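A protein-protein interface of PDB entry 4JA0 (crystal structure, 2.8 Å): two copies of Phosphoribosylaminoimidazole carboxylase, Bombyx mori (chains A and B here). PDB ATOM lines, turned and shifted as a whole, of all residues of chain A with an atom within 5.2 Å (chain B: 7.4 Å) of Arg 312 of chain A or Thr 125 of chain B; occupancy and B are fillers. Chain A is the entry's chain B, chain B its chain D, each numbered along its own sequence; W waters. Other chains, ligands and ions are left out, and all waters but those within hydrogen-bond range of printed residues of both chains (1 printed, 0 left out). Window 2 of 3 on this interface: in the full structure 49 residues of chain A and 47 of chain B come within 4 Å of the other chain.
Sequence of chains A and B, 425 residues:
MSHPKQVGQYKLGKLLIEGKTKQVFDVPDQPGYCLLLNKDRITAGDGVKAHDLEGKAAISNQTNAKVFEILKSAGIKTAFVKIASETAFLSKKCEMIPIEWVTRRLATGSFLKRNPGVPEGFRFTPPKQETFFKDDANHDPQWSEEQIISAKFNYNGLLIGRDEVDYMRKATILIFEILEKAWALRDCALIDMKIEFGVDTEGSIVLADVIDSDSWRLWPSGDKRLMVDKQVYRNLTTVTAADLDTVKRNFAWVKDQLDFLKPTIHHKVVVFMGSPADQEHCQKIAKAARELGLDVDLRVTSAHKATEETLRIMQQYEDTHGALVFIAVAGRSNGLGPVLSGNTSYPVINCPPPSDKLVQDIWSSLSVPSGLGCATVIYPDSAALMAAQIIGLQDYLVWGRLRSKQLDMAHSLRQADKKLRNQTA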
ATOM      1  N   GLU A 308      -6.406 -14.119 -32.605  1.00  0.00           N
ATOM      2  CA  GLU A 308      -6.632 -14.481 -31.210  1.00  0.00           C
ATOM      3  C   GLU A 308      -7.232 -15.896 -31.067  1.00  0.00           C
ATOM      4  O   GLU A 308      -6.891 -16.617 -30.144  1.00  0.00           O
ATOM      5  CB  GLU A 308      -7.512 -13.410 -30.534  1.00  0.00           C
ATOM      6  CG  GLU A 308      -8.996 -13.438 -30.963  1.00  0.00           C
ATOM      7  CD  GLU A 308      -9.222 -13.317 -32.488  1.00  0.00           C
ATOM      8  OE1 GLU A 308      -8.431 -12.631 -33.195  1.00  0.00           O
ATOM      9  OE2 GLU A 308     -10.183 -13.957 -32.984  1.00  0.00           O
ATOM     10  N   GLU A 309      -8.124 -16.294 -31.970  1.00  0.00           N
ATOM     11  CA  GLU A 309      -8.718 -17.622 -31.901  1.00  0.00           C
ATOM     12  C   GLU A 309      -7.713 -18.710 -32.332  1.00  0.00           C
ATOM     13  O   GLU A 309      -7.763 -19.854 -31.847  1.00  0.00           O
ATOM     14  CB  GLU A 309     -10.000 -17.677 -32.730  1.00  0.00           C
ATOM     15  CG  GLU A 309     -10.690 -19.058 -32.784  1.00  0.00           C
ATOM     16  CD  GLU A 309     -11.346 -19.532 -31.464  1.00  0.00           C
ATOM     17  OE1 GLU A 309     -11.340 -18.792 -30.449  1.00  0.00           O
ATOM     18  OE2 GLU A 309     -11.890 -20.665 -31.452  1.00  0.00           O
ATOM     19  N   THR A 310      -6.811 -18.360 -33.252  1.00  0.00           N
ATOM     20  CA  THR A 310      -5.730 -19.267 -33.618  1.00  0.00           C
ATOM     21  C   THR A 310      -4.910 -19.620 -32.391  1.00  0.00           C
ATOM     22  O   THR A 310      -4.710 -20.801 -32.094  1.00  0.00           O
ATOM     23  CB  THR A 310      -4.836 -18.660 -34.702  1.00  0.00           C
ATOM     24  OG1 THR A 310      -5.512 -18.762 -35.953  1.00  0.00           O
ATOM     25  CG2 THR A 310      -3.542 -19.414 -34.833  1.00  0.00           C
ATOM     26  N   LEU A 311      -4.489 -18.605 -31.638  1.00  0.00           N
ATOM     27  CA  LEU A 311      -3.769 -18.852 -30.389  1.00  0.00           C
ATOM     28  C   LEU A 311      -4.585 -19.661 -29.397  1.00  0.00           C
ATOM     29  O   LEU A 311      -4.049 -20.519 -28.694  1.00  0.00           O
ATOM     30  CB  LEU A 311      -3.340 -17.546 -29.742  1.00  0.00           C
ATOM     31  CG  LEU A 311      -2.314 -16.794 -30.581  1.00  0.00           C
ATOM     32  CD1 LEU A 311      -1.793 -15.626 -29.781  1.00  0.00           C
ATOM     33  CD2 LEU A 311      -1.176 -17.706 -31.046  1.00  0.00           C
ATOM     34  N   ARG A 312      -5.884 -19.396 -29.372  1.00  0.00           N
ATOM     35  CA  ARG A 312      -6.812 -20.052 -28.463  1.00  0.00           C
ATOM     36  C   ARG A 312      -6.949 -21.548 -28.737  1.00  0.00           C
ATOM     37  O   ARG A 312      -7.065 -22.356 -27.813  1.00  0.00           O
ATOM     38  CB  ARG A 312      -8.186 -19.380 -28.569  1.00  0.00           C
ATOM     39  CG  ARG A 312      -8.963 -19.367 -27.296  1.00  0.00           C
ATOM     40  CD  ARG A 312      -8.383 -18.349 -26.342  1.00  0.00           C
ATOM     41  NE  ARG A 312      -8.769 -18.672 -24.973  1.00  0.00           N
ATOM     42  CZ  ARG A 312      -8.783 -17.798 -23.974  1.00  0.00           C
ATOM     43  NH1 ARG A 312      -8.435 -16.534 -24.194  1.00  0.00           N
ATOM     44  NH2 ARG A 312      -9.150 -18.192 -22.761  1.00  0.00           N
ATOM     45  N   ILE A 313      -6.938 -21.907 -30.012  1.00  0.00           N
ATOM     46  CA  ILE A 313      -7.065 -23.300 -30.401  1.00  0.00           C
ATOM     47  C   ILE A 313      -5.796 -24.069 -30.042  1.00  0.00           C
ATOM     48  O   ILE A 313      -5.878 -25.201 -29.554  1.00  0.00           O
ATOM     49  CB  ILE A 313      -7.420 -23.417 -31.903  1.00  0.00           C
ATOM     50  CG1 ILE A 313      -8.786 -22.761 -32.144  1.00  0.00           C
ATOM     51  CG2 ILE A 313      -7.441 -24.849 -32.362  1.00  0.00           C
ATOM     52  CD1 ILE A 313      -9.339 -22.947 -33.514  1.00  0.00           C
ATOM     53  N   MET A 314      -4.621 -23.461 -30.216  1.00  0.00           N
ATOM     54  CA  MET A 314      -3.404 -24.195 -29.871  1.00  0.00           C
ATOM     55  C   MET A 314      -3.205 -24.366 -28.353  1.00  0.00           C
ATOM     56  O   MET A 314      -2.601 -25.347 -27.908  1.00  0.00           O
ATOM     57  CB  MET A 314      -2.157 -23.595 -30.541  1.00  0.00           C
ATOM     58  CG  MET A 314      -1.843 -22.161 -30.170  1.00  0.00           C
ATOM     59  SD  MET A 314      -0.092 -21.918 -29.812  1.00  0.00           S
ATOM     60  CE  MET A 314      -0.050 -22.797 -28.262  1.00  0.00           C
ATOM     61  N   GLN A 315      -3.744 -23.447 -27.556  1.00  0.00           N
ATOM     62  CA  GLN A 315      -3.670 -23.572 -26.099  1.00  0.00           C
ATOM     63  C   GLN A 315      -4.580 -24.679 -25.604  1.00  0.00           C
ATOM     64  O   GLN A 315      -4.370 -25.239 -24.533  1.00  0.00           O
ATOM     65  CB  GLN A 315      -3.996 -22.233 -25.429  1.00  0.00           C
ATOM     66  CG  GLN A 315      -2.801 -21.295 -25.420  1.00  0.00           C
ATOM     67  CD  GLN A 315      -3.173 -19.829 -25.364  1.00  0.00           C
ATOM     68  OE1 GLN A 315      -4.331 -19.436 -25.608  1.00  0.00           O
ATOM     69  NE2 GLN A 315      -2.168 -18.994 -25.104  1.00  0.00           N
ATOM     70  N   GLN A 316      -5.603 -24.991 -26.384  1.00  0.00           N
ATOM     71  CA  GLN A 316      -6.474 -26.096 -26.040  1.00  0.00           C
ATOM     72  C   GLN A 316      -5.765 -27.418 -26.287  1.00  0.00           C
ATOM     73  O   GLN A 316      -5.900 -28.369 -25.523  1.00  0.00           O
ATOM     74  CB  GLN A 316      -7.774 -25.997 -26.826  1.00  0.00           C
ATOM     75  CG  GLN A 316      -8.610 -24.766 -26.422  1.00  0.00           C
ATOM     76  CD  GLN A 316      -9.738 -24.499 -27.391  1.00  0.00           C
ATOM     77  OE1 GLN A 316      -9.855 -25.163 -28.432  1.00  0.00           O
ATOM     78  NE2 GLN A 316     -10.537 -23.474 -27.098  1.00  0.00           N
ATOM     79  N   ASP A 319      -3.087 -28.345 -23.461  1.00  0.00           N
ATOM     80  CA  ASP A 319      -3.541 -28.986 -22.239  1.00  0.00           C
ATOM     81  C   ASP A 319      -3.469 -30.514 -22.424  1.00  0.00           C
ATOM     82  O   ASP A 319      -4.490 -31.177 -22.597  1.00  0.00           O
ATOM     83  CB  ASP A 319      -4.973 -28.522 -21.936  1.00  0.00           C
ATOM     84  CG  ASP A 319      -5.541 -29.078 -20.610  1.00  0.00           C
ATOM     85  OD1 ASP A 319      -4.768 -29.517 -19.715  1.00  0.00           O
ATOM     86  OD2 ASP A 319      -6.789 -29.048 -20.463  1.00  0.00           O
ATOM     87  N   ARG B 104      -4.805 -21.216 -12.205  1.00  0.00           N
ATOM     88  CA  ARG B 104      -5.624 -22.419 -12.110  1.00  0.00           C
ATOM     89  C   ARG B 104      -5.729 -23.116 -13.451  1.00  0.00           C
ATOM     90  O   ARG B 104      -5.799 -22.468 -14.491  1.00  0.00           O
ATOM     91  CB  ARG B 104      -7.053 -22.092 -11.664  1.00  0.00           C
ATOM     92  CG  ARG B 104      -7.154 -21.105 -10.538  1.00  0.00           C
ATOM     93  CD  ARG B 104      -8.611 -20.869 -10.167  1.00  0.00           C
ATOM     94  NE  ARG B 104      -8.764 -19.694  -9.317  1.00  0.00           N
ATOM     95  CZ  ARG B 104      -8.593 -19.686  -7.997  1.00  0.00           C
ATOM     96  NH1 ARG B 104      -8.247 -20.803  -7.363  1.00  0.00           N
ATOM     97  NH2 ARG B 104      -8.755 -18.550  -7.320  1.00  0.00           N
ATOM     98  N   ARG B 105      -5.778 -24.443 -13.422  1.00  0.00           N
ATOM     99  CA  ARG B 105      -6.084 -25.207 -14.629  1.00  0.00           C
ATOM    100  C   ARG B 105      -7.548 -25.657 -14.571  1.00  0.00           C
ATOM    101  O   ARG B 105      -8.192 -25.857 -15.599  1.00  0.00           O
ATOM    102  CB  ARG B 105      -5.146 -26.407 -14.748  1.00  0.00           C
ATOM    103  CG  ARG B 105      -5.515 -27.379 -15.858  1.00  0.00           C
ATOM    104  CD  ARG B 105      -5.319 -26.784 -17.249  1.00  0.00           C
ATOM    105  NE  ARG B 105      -3.903 -26.806 -17.610  1.00  0.00           N
ATOM    106  CZ  ARG B 105      -3.393 -26.258 -18.702  1.00  0.00           C
ATOM    107  NH1 ARG B 105      -4.183 -25.636 -19.564  1.00  0.00           N
ATOM    108  NH2 ARG B 105      -2.088 -26.337 -18.925  1.00  0.00           N
ATOM    109  N   PHE B 122     -14.046 -27.746 -14.294  1.00  0.00           N
ATOM    110  CA  PHE B 122     -14.059 -26.969 -15.518  1.00  0.00           C
ATOM    111  C   PHE B 122     -12.629 -26.592 -15.829  1.00  0.00           C
ATOM    112  O   PHE B 122     -11.926 -26.029 -14.986  1.00  0.00           O
ATOM    113  CB  PHE B 122     -14.919 -25.709 -15.375  1.00  0.00           C
ATOM    114  CG  PHE B 122     -14.928 -24.853 -16.601  1.00  0.00           C
ATOM    115  CD1 PHE B 122     -15.940 -24.990 -17.544  1.00  0.00           C
ATOM    116  CD2 PHE B 122     -13.917 -23.920 -16.830  1.00  0.00           C
ATOM    117  CE1 PHE B 122     -15.952 -24.202 -18.700  1.00  0.00           C
ATOM    118  CE2 PHE B 122     -13.916 -23.124 -17.979  1.00  0.00           C
ATOM    119  CZ  PHE B 122     -14.936 -23.268 -18.916  1.00  0.00           C
ATOM    120  N   ARG B 123     -12.197 -26.931 -17.034  1.00  0.00           N
ATOM    121  CA  ARG B 123     -10.792 -26.796 -17.396  1.00  0.00           C
ATOM    122  C   ARG B 123     -10.511 -25.464 -18.070  1.00  0.00           C
ATOM    123  O   ARG B 123     -11.265 -25.020 -18.940  1.00  0.00           O
ATOM    124  CB  ARG B 123     -10.318 -27.966 -18.274  1.00  0.00           C
ATOM    125  CG  ARG B 123     -10.357 -29.327 -17.610  1.00  0.00           C
ATOM    126  CD  ARG B 123      -9.534 -30.337 -18.391  1.00  0.00           C
ATOM    127  NE  ARG B 123      -8.087 -30.169 -18.176  1.00  0.00           N
ATOM    128  CZ  ARG B 123      -7.386 -30.717 -17.179  1.00  0.00           C
ATOM    129  NH1 ARG B 123      -7.973 -31.494 -16.284  1.00  0.00           N
ATOM    130  NH2 ARG B 123      -6.083 -30.505 -17.080  1.00  0.00           N
ATOM    131  N   PHE B 124      -9.421 -24.832 -17.645  1.00  0.00           N
ATOM    132  CA  PHE B 124      -9.000 -23.538 -18.171  1.00  0.00           C
ATOM    133  C   PHE B 124      -7.859 -23.688 -19.172  1.00  0.00           C
ATOM    134  O   PHE B 124      -6.724 -24.020 -18.791  1.00  0.00           O
ATOM    135  CB  PHE B 124      -8.535 -22.625 -17.029  1.00  0.00           C
ATOM    136  CG  PHE B 124      -9.633 -22.215 -16.095  1.00  0.00           C
ATOM    137  CD1 PHE B 124      -9.584 -22.563 -14.748  1.00  0.00           C
ATOM    138  CD2 PHE B 124     -10.731 -21.493 -16.567  1.00  0.00           C
ATOM    139  CE1 PHE B 124     -10.596 -22.190 -13.893  1.00  0.00           C
ATOM    140  CE2 PHE B 124     -11.743 -21.107 -15.718  1.00  0.00           C
ATOM    141  CZ  PHE B 124     -11.680 -21.462 -14.376  1.00  0.00           C
ATOM    142  N   THR B 125      -8.149 -23.430 -20.445  1.00  0.00           N
ATOM    143  CA  THR B 125      -7.112 -23.463 -21.484  1.00  0.00           C
ATOM    144  C   THR B 125      -7.189 -22.119 -22.217  1.00  0.00           C
ATOM    145  O   THR B 125      -8.211 -21.804 -22.838  1.00  0.00           O
ATOM    146  CB  THR B 125      -7.265 -24.683 -22.445  1.00  0.00           C
ATOM    147  OG1 THR B 125      -8.486 -24.581 -23.182  1.00  0.00           O
ATOM    148  CG2 THR B 125      -7.311 -25.968 -21.670  1.00  0.00           C
ATOM    149  N   PRO B 126      -6.162 -21.260 -22.050  1.00  0.00           N
ATOM    150  CA  PRO B 126      -4.921 -21.432 -21.284  1.00  0.00           C
ATOM    151  C   PRO B 126      -5.199 -21.337 -19.783  1.00  0.00           C
ATOM    152  O   PRO B 126      -6.324 -21.030 -19.382  1.00  0.00           O
ATOM    153  CB  PRO B 126      -4.062 -20.243 -21.758  1.00  0.00           C
ATOM    154  CG  PRO B 126      -5.037 -19.197 -22.082  1.00  0.00           C
ATOM    155  CD  PRO B 126      -6.239 -19.912 -22.650  1.00  0.00           C
ATOM    156  N   PRO B 127      -4.197 -21.627 -18.949  1.00  0.00           N
ATOM    157  CA  PRO B 127      -4.530 -21.573 -17.524  1.00  0.00           C
ATOM    158  C   PRO B 127      -4.989 -20.193 -17.069  1.00  0.00           C
ATOM    159  O   PRO B 127      -4.367 -19.191 -17.417  1.00  0.00           O
ATOM    160  CB  PRO B 127      -3.206 -21.942 -16.849  1.00  0.00           C
ATOM    161  CG  PRO B 127      -2.457 -22.760 -17.891  1.00  0.00           C
ATOM    162  CD  PRO B 127      -2.825 -22.114 -19.192  1.00  0.00           C
ATOM    163  N   LYS B 128      -6.049 -20.144 -16.273  1.00  0.00           N
ATOM    164  CA  LYS B 128      -6.510 -18.882 -15.729  1.00  0.00           C
ATOM    165  C   LYS B 128      -5.476 -18.301 -14.803  1.00  0.00           C
ATOM    166  O   LYS B 128      -4.862 -19.028 -14.014  1.00  0.00           O
ATOM    167  CB  LYS B 128      -7.781 -19.085 -14.925  1.00  0.00           C
ATOM    168  CG  LYS B 128      -9.000 -18.607 -15.644  1.00  0.00           C
ATOM    169  CD  LYS B 128      -9.969 -17.931 -14.721  1.00  0.00           C
ATOM    170  CE  LYS B 128     -11.063 -17.317 -15.575  1.00  0.00           C
ATOM    171  NZ  LYS B 128     -10.430 -16.642 -16.758  1.00  0.00           N
HETATM  172  O   HOH W   1      -3.752 -24.587 -21.878  1.00  0.00           O
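The side-chain carboxylate of Asp 319 of chain A lies within salt-bridge range of the guanidinium group of Arg 123 of chain B (2.9 Å).
OD1 of Asp 319 of chain A is in salt-bridge range of NE of Arg 105 of chain B (3.5 Å).
The backbone carbonyl oxygen of Leu 311 of chain A sits close to the side-chain amide oxygen of Gln 315 of chain A, 3.3 Å away.
O of Arg 105 of chain B lies within hydrogen-bond range of N of Phe 124 of chain B (2.6 Å).
Thr 310 of chain A touches none of the printed residues of chain B.
Printed residues of chain B within 4 Å of Arg 312 of chain A: Thr 125 (3.7 Å) and Pro 126 (3.4 Å).
Of the printed residues of chain B, Gln 315 of chain A touches Thr 125 (3.6 Å) and Pro 126 (3.6 Å).
Of the printed residues of chain A, Arg 123 of chain B touches Asp 319 (2.9 Å).
Of the printed residues of chain A, Thr 125 of chain B touches Arg 312, Gln 315, Gln 316 and Asp 319.
Pro 127 of chain B touches none of the printed residues of chain A.
Among the printed residues, pairs that only touch across the chains: Arg 312 of chain A with Thr 125 of chain B, Arg 312 of chain A with Pro 126 of chain B, Gln 315 of chain A with Thr 125 of chain B, Gln 315 of chain A with Pro 126 of chain B, Gln 316 of chain A with Thr 125 of chain B and Asp 319 of chain A with Thr 125 of chain B.
No position is printed for both chains.
Of the 8 pairs that touch across the chains among the printed residues, none has its exchanged pair printed and touching as well.
Of the 9 printed residues of chain B, 4 touch a printed residue of chain A.
Hydrophobic or aromatic side chains of chain B within 4 Å of the printed part of chain A: Pro 126.
Among the printed residues, Asp or Glu carboxylates within 4 Å of a Lys or Arg side-chain nitrogen of the other chain: Asp 319 of chain A with Arg 105 of chain B (3.5 Å) and Asp 319 of chain A with Arg 123 of chain B (2.9 Å).
Water W1 bridges the guanidinium group of Arg 105 of chain B and the backbone carbonyl oxygen of Gln 315 of chain A.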
